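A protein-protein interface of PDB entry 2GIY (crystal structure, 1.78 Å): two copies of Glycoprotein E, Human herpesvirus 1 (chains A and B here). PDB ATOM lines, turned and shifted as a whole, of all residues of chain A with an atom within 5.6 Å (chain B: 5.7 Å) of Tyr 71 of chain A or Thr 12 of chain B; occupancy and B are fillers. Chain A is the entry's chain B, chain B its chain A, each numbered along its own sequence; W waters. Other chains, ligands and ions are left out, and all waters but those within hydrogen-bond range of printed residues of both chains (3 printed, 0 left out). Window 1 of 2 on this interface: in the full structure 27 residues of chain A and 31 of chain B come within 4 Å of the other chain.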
ATOM      1  N   GLU A  67     -24.207  -0.538   9.874  1.00  0.00           N
ATOM      2  CA  GLU A  67     -23.776   0.692  10.527  1.00  0.00           C
ATOM      3  C   GLU A  67     -23.863   1.942   9.660  1.00  0.00           C
ATOM      4  O   GLU A  67     -24.441   2.943  10.077  1.00  0.00           O
ATOM      5  CB  GLU A  67     -22.352   0.535  11.060  1.00  0.00           C
ATOM      6  CG  GLU A  67     -21.764   1.820  11.631  1.00  0.00           C
ATOM      7  CD  GLU A  67     -20.532   1.564  12.463  1.00  0.00           C
ATOM      8  OE1 GLU A  67     -19.654   0.808  12.004  1.00  0.00           O
ATOM      9  OE2 GLU A  67     -20.441   2.119  13.578  1.00  0.00           O
ATOM     10  N   SER A  68     -23.291   1.890   8.462  1.00  0.00           N
ATOM     11  CA  SER A  68     -23.314   3.041   7.568  1.00  0.00           C
ATOM     12  C   SER A  68     -24.732   3.504   7.283  1.00  0.00           C
ATOM     13  O   SER A  68     -24.992   4.699   7.148  1.00  0.00           O
ATOM     14  CB  SER A  68     -22.605   2.707   6.251  1.00  0.00           C
ATOM     15  OG  SER A  68     -21.228   2.457   6.468  1.00  0.00           O
ATOM     16  N   CYS A  69     -25.652   2.550   7.194  1.00  0.00           N
ATOM     17  CA  CYS A  69     -27.041   2.869   6.917  1.00  0.00           C
ATOM     18  C   CYS A  69     -27.721   3.686   8.011  1.00  0.00           C
ATOM     19  O   CYS A  69     -28.670   4.416   7.742  1.00  0.00           O
ATOM     20  CB  CYS A  69     -27.831   1.585   6.674  1.00  0.00           C
ATOM     21  SG  CYS A  69     -27.585   0.892   5.011  1.00  0.00           S
ATOM     22  N   LEU A  70     -27.243   3.562   9.243  1.00  0.00           N
ATOM     23  CA  LEU A  70     -27.843   4.307  10.343  1.00  0.00           C
ATOM     24  C   LEU A  70     -27.797   5.808  10.083  1.00  0.00           C
ATOM     25  O   LEU A  70     -28.734   6.531  10.419  1.00  0.00           O
ATOM     26  CB  LEU A  70     -27.131   3.981  11.663  1.00  0.00           C
ATOM     27  CG  LEU A  70     -27.208   2.528  12.145  1.00  0.00           C
ATOM     28  CD1 LEU A  70     -26.504   2.406  13.488  1.00  0.00           C
ATOM     29  CD2 LEU A  70     -28.663   2.091  12.269  1.00  0.00           C
ATOM     30  N   TYR A  71     -26.710   6.275   9.475  1.00  0.00           N
ATOM     31  CA  TYR A  71     -26.563   7.697   9.182  1.00  0.00           C
ATOM     32  C   TYR A  71     -27.352   8.117   7.942  1.00  0.00           C
ATOM     33  O   TYR A  71     -27.690   9.290   7.786  1.00  0.00           O
ATOM     34  CB  TYR A  71     -25.081   8.056   8.999  1.00  0.00           C
ATOM     35  CG  TYR A  71     -24.219   7.654  10.175  1.00  0.00           C
ATOM     36  CD1 TYR A  71     -23.756   6.348  10.309  1.00  0.00           C
ATOM     37  CD2 TYR A  71     -23.922   8.565  11.190  1.00  0.00           C
ATOM     38  CE1 TYR A  71     -23.020   5.953  11.427  1.00  0.00           C
ATOM     39  CE2 TYR A  71     -23.191   8.181  12.311  1.00  0.00           C
ATOM     40  CZ  TYR A  71     -22.745   6.875  12.425  1.00  0.00           C
ATOM     41  OH  TYR A  71     -22.039   6.485  13.544  1.00  0.00           O
ATOM     42  N   HIS A  72     -27.656   7.157   7.075  1.00  0.00           N
ATOM     43  CA  HIS A  72     -28.404   7.432   5.845  1.00  0.00           C
ATOM     44  C   HIS A  72     -29.404   6.312   5.570  1.00  0.00           C
ATOM     45  O   HIS A  72     -29.286   5.591   4.578  1.00  0.00           O
ATOM     46  CB  HIS A  72     -27.435   7.547   4.667  1.00  0.00           C
ATOM     47  CG  HIS A  72     -26.416   8.631   4.829  1.00  0.00           C
ATOM     48  ND1 HIS A  72     -26.748   9.969   4.837  1.00  0.00           N
ATOM     49  CD2 HIS A  72     -25.074   8.575   5.001  1.00  0.00           C
ATOM     50  CE1 HIS A  72     -25.654  10.691   5.005  1.00  0.00           C
ATOM     51  NE2 HIS A  72     -24.624   9.868   5.107  1.00  0.00           N
ATOM     52  N   PRO A  73     -30.415   6.164   6.440  1.00  0.00           N
ATOM     53  CA  PRO A  73     -31.436   5.121   6.296  1.00  0.00           C
ATOM     54  C   PRO A  73     -32.380   5.272   5.103  1.00  0.00           C
ATOM     55  O   PRO A  73     -33.259   4.435   4.894  1.00  0.00           O
ATOM     56  CB  PRO A  73     -32.164   5.173   7.638  1.00  0.00           C
ATOM     57  CG  PRO A  73     -32.103   6.629   7.988  1.00  0.00           C
ATOM     58  CD  PRO A  73     -30.677   6.999   7.629  1.00  0.00           C
ATOM     59  N   HIS A 155     -27.601  15.023  14.157  1.00  0.00           N
ATOM     60  CA  HIS A 155     -26.577  14.136  13.616  1.00  0.00           C
ATOM     61  C   HIS A 155     -26.230  13.088  14.660  1.00  0.00           C
ATOM     62  O   HIS A 155     -26.034  13.419  15.827  1.00  0.00           O
ATOM     63  CB  HIS A 155     -25.322  14.928  13.242  1.00  0.00           C
ATOM     64  CG  HIS A 155     -24.138  14.068  12.924  1.00  0.00           C
ATOM     65  ND1 HIS A 155     -24.184  13.049  11.996  1.00  0.00           N
ATOM     66  CD2 HIS A 155     -22.873  14.077  13.409  1.00  0.00           C
ATOM     67  CE1 HIS A 155     -22.999  12.470  11.922  1.00  0.00           C
ATOM     68  NE2 HIS A 155     -22.186  13.075  12.769  1.00  0.00           N
ATOM     69  N   ILE A 156     -26.153  11.824  14.252  1.00  0.00           N
ATOM     70  CA  ILE A 156     -25.831  10.764  15.201  1.00  0.00           C
ATOM     71  C   ILE A 156     -24.449  10.972  15.820  1.00  0.00           C
ATOM     72  O   ILE A 156     -23.454  11.088  15.103  1.00  0.00           O
ATOM     73  CB  ILE A 156     -25.868   9.371  14.530  1.00  0.00           C
ATOM     74  CG1 ILE A 156     -27.264   9.100  13.966  1.00  0.00           C
ATOM     75  CG2 ILE A 156     -25.486   8.304  15.538  1.00  0.00           C
ATOM     76  CD1 ILE A 156     -27.420   7.733  13.318  1.00  0.00           C
ATOM     77  N   TRP A 159     -24.337   5.564  19.287  1.00  0.00           N
ATOM     78  CA  TRP A 159     -25.393   4.579  19.126  1.00  0.00           C
ATOM     79  C   TRP A 159     -24.919   3.254  19.685  1.00  0.00           C
ATOM     80  O   TRP A 159     -23.715   3.013  19.831  1.00  0.00           O
ATOM     81  CB  TRP A 159     -25.786   4.403  17.652  1.00  0.00           C
ATOM     82  CG  TRP A 159     -24.786   3.639  16.831  1.00  0.00           C
ATOM     83  CD1 TRP A 159     -23.684   4.140  16.201  1.00  0.00           C
ATOM     84  CD2 TRP A 159     -24.797   2.231  16.564  1.00  0.00           C
ATOM     85  NE1 TRP A 159     -23.009   3.133  15.553  1.00  0.00           N
ATOM     86  CE2 TRP A 159     -23.670   1.950  15.759  1.00  0.00           C
ATOM     87  CE3 TRP A 159     -25.652   1.179  16.924  1.00  0.00           C
ATOM     88  CZ2 TRP A 159     -23.372   0.659  15.308  1.00  0.00           C
ATOM     89  CZ3 TRP A 159     -25.355  -0.109  16.474  1.00  0.00           C
ATOM     90  CH2 TRP A 159     -24.224  -0.355  15.674  1.00  0.00           C
ATOM     91  N   VAL B   8     -25.659  15.759   8.711  1.00  0.00           N
ATOM     92  CA  VAL B   8     -24.677  14.694   8.874  1.00  0.00           C
ATOM     93  C   VAL B   8     -23.353  15.115   8.241  1.00  0.00           C
ATOM     94  O   VAL B   8     -23.236  15.184   7.018  1.00  0.00           O
ATOM     95  CB  VAL B   8     -25.168  13.392   8.212  1.00  0.00           C
ATOM     96  CG1 VAL B   8     -24.155  12.277   8.428  1.00  0.00           C
ATOM     97  CG2 VAL B   8     -26.524  13.007   8.782  1.00  0.00           C
ATOM     98  N   GLY B  10     -18.700  15.756   9.157  1.00  0.00           N
ATOM     99  CA  GLY B  10     -17.558  15.439   9.993  1.00  0.00           C
ATOM    100  C   GLY B  10     -17.160  13.978   9.925  1.00  0.00           C
ATOM    101  O   GLY B  10     -17.472  13.275   8.961  1.00  0.00           O
ATOM    102  N   VAL B  11     -16.465  13.519  10.962  1.00  0.00           N
ATOM    103  CA  VAL B  11     -16.000  12.142  11.026  1.00  0.00           C
ATOM    104  C   VAL B  11     -16.466  11.466  12.308  1.00  0.00           C
ATOM    105  O   VAL B  11     -16.525  12.097  13.361  1.00  0.00           O
ATOM    106  CB  VAL B  11     -14.455  12.078  10.988  1.00  0.00           C
ATOM    107  CG1 VAL B  11     -13.990  10.624  10.937  1.00  0.00           C
ATOM    108  CG2 VAL B  11     -13.930  12.861   9.793  1.00  0.00           C
ATOM    109  N   THR B  12     -16.807  10.184  12.205  1.00  0.00           N
ATOM    110  CA  THR B  12     -17.225   9.408  13.364  1.00  0.00           C
ATOM    111  C   THR B  12     -16.183   8.324  13.611  1.00  0.00           C
ATOM    112  O   THR B  12     -15.820   7.590  12.697  1.00  0.00           O
ATOM    113  CB  THR B  12     -18.589   8.724  13.140  1.00  0.00           C
ATOM    114  OG1 THR B  12     -19.622   9.714  13.114  1.00  0.00           O
ATOM    115  CG2 THR B  12     -18.872   7.727  14.255  1.00  0.00           C
ATOM    116  N   VAL B  13     -15.695   8.236  14.843  1.00  0.00           N
ATOM    117  CA  VAL B  13     -14.712   7.221  15.185  1.00  0.00           C
ATOM    118  C   VAL B  13     -15.259   6.339  16.295  1.00  0.00           C
ATOM    119  O   VAL B  13     -15.740   6.836  17.315  1.00  0.00           O
ATOM    120  CB  VAL B  13     -13.384   7.844  15.656  1.00  0.00           C
ATOM    121  CG1 VAL B  13     -12.374   6.736  15.968  1.00  0.00           C
ATOM    122  CG2 VAL B  13     -12.833   8.779  14.585  1.00  0.00           C
ATOM    123  N   ARG B  14     -15.192   5.029  16.085  1.00  0.00           N
ATOM    124  CA  ARG B  14     -15.675   4.066  17.065  1.00  0.00           C
ATOM    125  C   ARG B  14     -14.498   3.183  17.462  1.00  0.00           C
ATOM    126  O   ARG B  14     -13.754   2.721  16.602  1.00  0.00           O
ATOM    127  CB  ARG B  14     -16.799   3.217  16.459  1.00  0.00           C
ATOM    128  CG  ARG B  14     -17.579   2.405  17.482  1.00  0.00           C
ATOM    129  CD  ARG B  14     -18.790   1.694  16.877  1.00  0.00           C
ATOM    130  NE  ARG B  14     -18.431   0.514  16.092  1.00  0.00           N
ATOM    131  CZ  ARG B  14     -17.997   0.541  14.835  1.00  0.00           C
ATOM    132  NH1 ARG B  14     -17.864   1.695  14.195  1.00  0.00           N
ATOM    133  NH2 ARG B  14     -17.692  -0.590  14.216  1.00  0.00           N
ATOM    134  N   HIS B  36     -12.649   2.095  13.946  1.00  0.00           N
ATOM    135  CA  HIS B  36     -13.281   2.337  12.660  1.00  0.00           C
ATOM    136  C   HIS B  36     -13.548   3.824  12.520  1.00  0.00           C
ATOM    137  O   HIS B  36     -13.945   4.488  13.474  1.00  0.00           O
ATOM    138  CB  HIS B  36     -14.601   1.570  12.563  1.00  0.00           C
ATOM    139  CG  HIS B  36     -14.433   0.084  12.533  1.00  0.00           C
ATOM    140  ND1 HIS B  36     -14.411  -0.640  11.360  1.00  0.00           N
ATOM    141  CD2 HIS B  36     -14.256  -0.813  13.531  1.00  0.00           C
ATOM    142  CE1 HIS B  36     -14.227  -1.918  11.638  1.00  0.00           C
ATOM    143  NE2 HIS B  36     -14.131  -2.050  12.949  1.00  0.00           N
ATOM    144  N   ALA B  37     -13.318   4.346  11.323  1.00  0.00           N
ATOM    145  CA  ALA B  37     -13.555   5.755  11.064  1.00  0.00           C
ATOM    146  C   ALA B  37     -14.514   5.865   9.890  1.00  0.00           C
ATOM    147  O   ALA B  37     -14.361   5.163   8.890  1.00  0.00           O
ATOM    148  CB  ALA B  37     -12.238   6.464  10.748  1.00  0.00           C
ATOM    149  N   ILE B  38     -15.512   6.731  10.022  1.00  0.00           N
ATOM    150  CA  ILE B  38     -16.487   6.938   8.959  1.00  0.00           C
ATOM    151  C   ILE B  38     -16.559   8.426   8.638  1.00  0.00           C
ATOM    152  O   ILE B  38     -16.979   9.225   9.473  1.00  0.00           O
ATOM    153  CB  ILE B  38     -17.901   6.453   9.372  1.00  0.00           C
ATOM    154  CG1 ILE B  38     -17.875   4.958   9.694  1.00  0.00           C
ATOM    155  CG2 ILE B  38     -18.892   6.726   8.245  1.00  0.00           C
ATOM    156  CD1 ILE B  38     -19.232   4.383  10.070  1.00  0.00           C
ATOM    157  N   ALA B  39     -16.127   8.800   7.438  1.00  0.00           N
ATOM    158  CA  ALA B  39     -16.177  10.200   7.020  1.00  0.00           C
ATOM    159  C   ALA B  39     -17.544  10.422   6.385  1.00  0.00           C
ATOM    160  O   ALA B  39     -17.892   9.755   5.414  1.00  0.00           O
ATOM    161  CB  ALA B  39     -15.069  10.497   6.014  1.00  0.00           C
ATOM    162  N   HIS B  40     -18.315  11.358   6.932  1.00  0.00           N
ATOM    163  CA  HIS B  40     -19.664  11.633   6.436  1.00  0.00           C
ATOM    164  C   HIS B  40     -19.736  12.635   5.287  1.00  0.00           C
ATOM    165  O   HIS B  40     -20.788  12.805   4.670  1.00  0.00           O
ATOM    166  CB  HIS B  40     -20.545  12.099   7.596  1.00  0.00           C
ATOM    167  CG  HIS B  40     -20.581  11.135   8.741  1.00  0.00           C
ATOM    168  ND1 HIS B  40     -21.027   9.837   8.607  1.00  0.00           N
ATOM    169  CD2 HIS B  40     -20.190  11.265  10.032  1.00  0.00           C
ATOM    170  CE1 HIS B  40     -20.906   9.211   9.764  1.00  0.00           C
ATOM    171  NE2 HIS B  40     -20.401  10.054  10.644  1.00  0.00           N
ATOM    172  N   HIS B 157     -11.917  12.146  19.164  1.00  0.00           N
ATOM    173  CA  HIS B 157     -13.152  11.597  18.607  1.00  0.00           C
ATOM    174  C   HIS B 157     -13.509  10.244  19.201  1.00  0.00           C
ATOM    175  O   HIS B 157     -14.616   9.745  19.011  1.00  0.00           O
ATOM    176  CB  HIS B 157     -13.058  11.489  17.083  1.00  0.00           C
ATOM    177  CG  HIS B 157     -13.291  12.789  16.384  1.00  0.00           C
ATOM    178  ND1 HIS B 157     -14.174  12.923  15.334  1.00  0.00           N
ATOM    179  CD2 HIS B 157     -12.792  14.026  16.616  1.00  0.00           C
ATOM    180  CE1 HIS B 157     -14.209  14.187  14.951  1.00  0.00           C
ATOM    181  NE2 HIS B 157     -13.381  14.877  15.713  1.00  0.00           N
HETATM  182  O   HOH W   1     -19.505  12.974  13.431  1.00  0.00           O
HETATM  183  O   HOH W   2     -22.077   8.663   6.205  1.00  0.00           O
HETATM  184  O   HOH W   3     -20.905   9.614  15.433  1.00  0.00           O
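NH1 of Arg 14 of chain B lies within salt-bridge range of OE2 of Glu 67 of chain A.
The backbone carbonyl oxygen (O) of Gly 10 of chain B lies within hydrogen-bond range of the backbone NH (N) of His 40 of chain B.
The backbone NH of Ile 38 of chain B is in hydrogen-bond range of the backbone carbonyl oxygen of Thr 12 of chain B, at 2.8 Å.
A ring nitrogen (NE2) of His 40 of chain B is in hydrogen-bond range of the side-chain hydroxyl (OG1) of Thr 12 of chain B, at 2.6 Å.
The backbone carbonyl oxygen (O) of His 36 of chain B sits at hydrogen-bond distance from the backbone NH (N) of Arg 14 of chain B.
The side-chain carboxylate of Glu 67 of chain A sits at hydrogen-bond distance from the indole nitrogen of Trp 159 of chain A (3.4 Å).
Among the printed residues, merely in contact across the chains: Glu 67 of chain A with Ile 38 of chain B (3.9 Å), Tyr 71 of chain A with Thr 12 of chain B (3.5 Å), Tyr 71 of chain A with His 40 of chain B (3.4 Å), His 155 of chain A with Val 8 of chain B (3.6 Å) and His 155 of chain A with His 40 of chain B (3.6 Å).
Thr 12 of chain B touches just one residue of chain A: Tyr 71.
Of the printed residues of chain B, Glu 67 of chain A touches Arg 14 and Ile 38.
Printed residues of chain B within 4 Å of His 155 of chain A: Val 8 and His 40.
His 72 of chain A touches none of the printed residues of chain B.
Val 11 of chain B touches none of the printed residues of chain A.
The nearest printed residue of chain A that does not touch Val 8 of chain B is Tyr 71 of chain A (4.02 Å).
Hydrophobic or aromatic side chains of chain B within 4 Å of the printed part of chain A: Val 8, Ile 38 and His 40.
Of the 10 printed residues of chain A, 3 touch a printed residue of chain B.
Hydrophobic or aromatic side chains of chain A within 4 Å of the printed part of chain B: Tyr 71 and His 155.
Among the printed residues, 6 pairs touch across the chains.
Among the printed residues, Asp or Glu carboxylates within 4 Å of a Lys or Arg side-chain nitrogen of the other chain: Glu 67 of chain A with Arg 14 of chain B (2.7 Å).
No position is printed for both chains.
Of the 6 pairs that touch across the chains among the printed residues, none has its exchanged pair printed and touching as well.
Water W3 lies within hydrogen-bond range of OG1 of Thr 12 of chain B and O of Ile 156 of chain A.
Water W1 lies within hydrogen-bond range of a ring nitrogen (NE2) of His 155 of chain A (2.8 Å), the backbone carbonyl oxygen of Val 11 of chain B (3.1 Å) and the side-chain hydroxyl of Thr 12 of chain B (3.3 Å).
Water W2 lies within hydrogen-bond range of ND1 of His 40 of chain B (2.9 Å) and NE2 of His 72 of chain A (3.0 Å).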
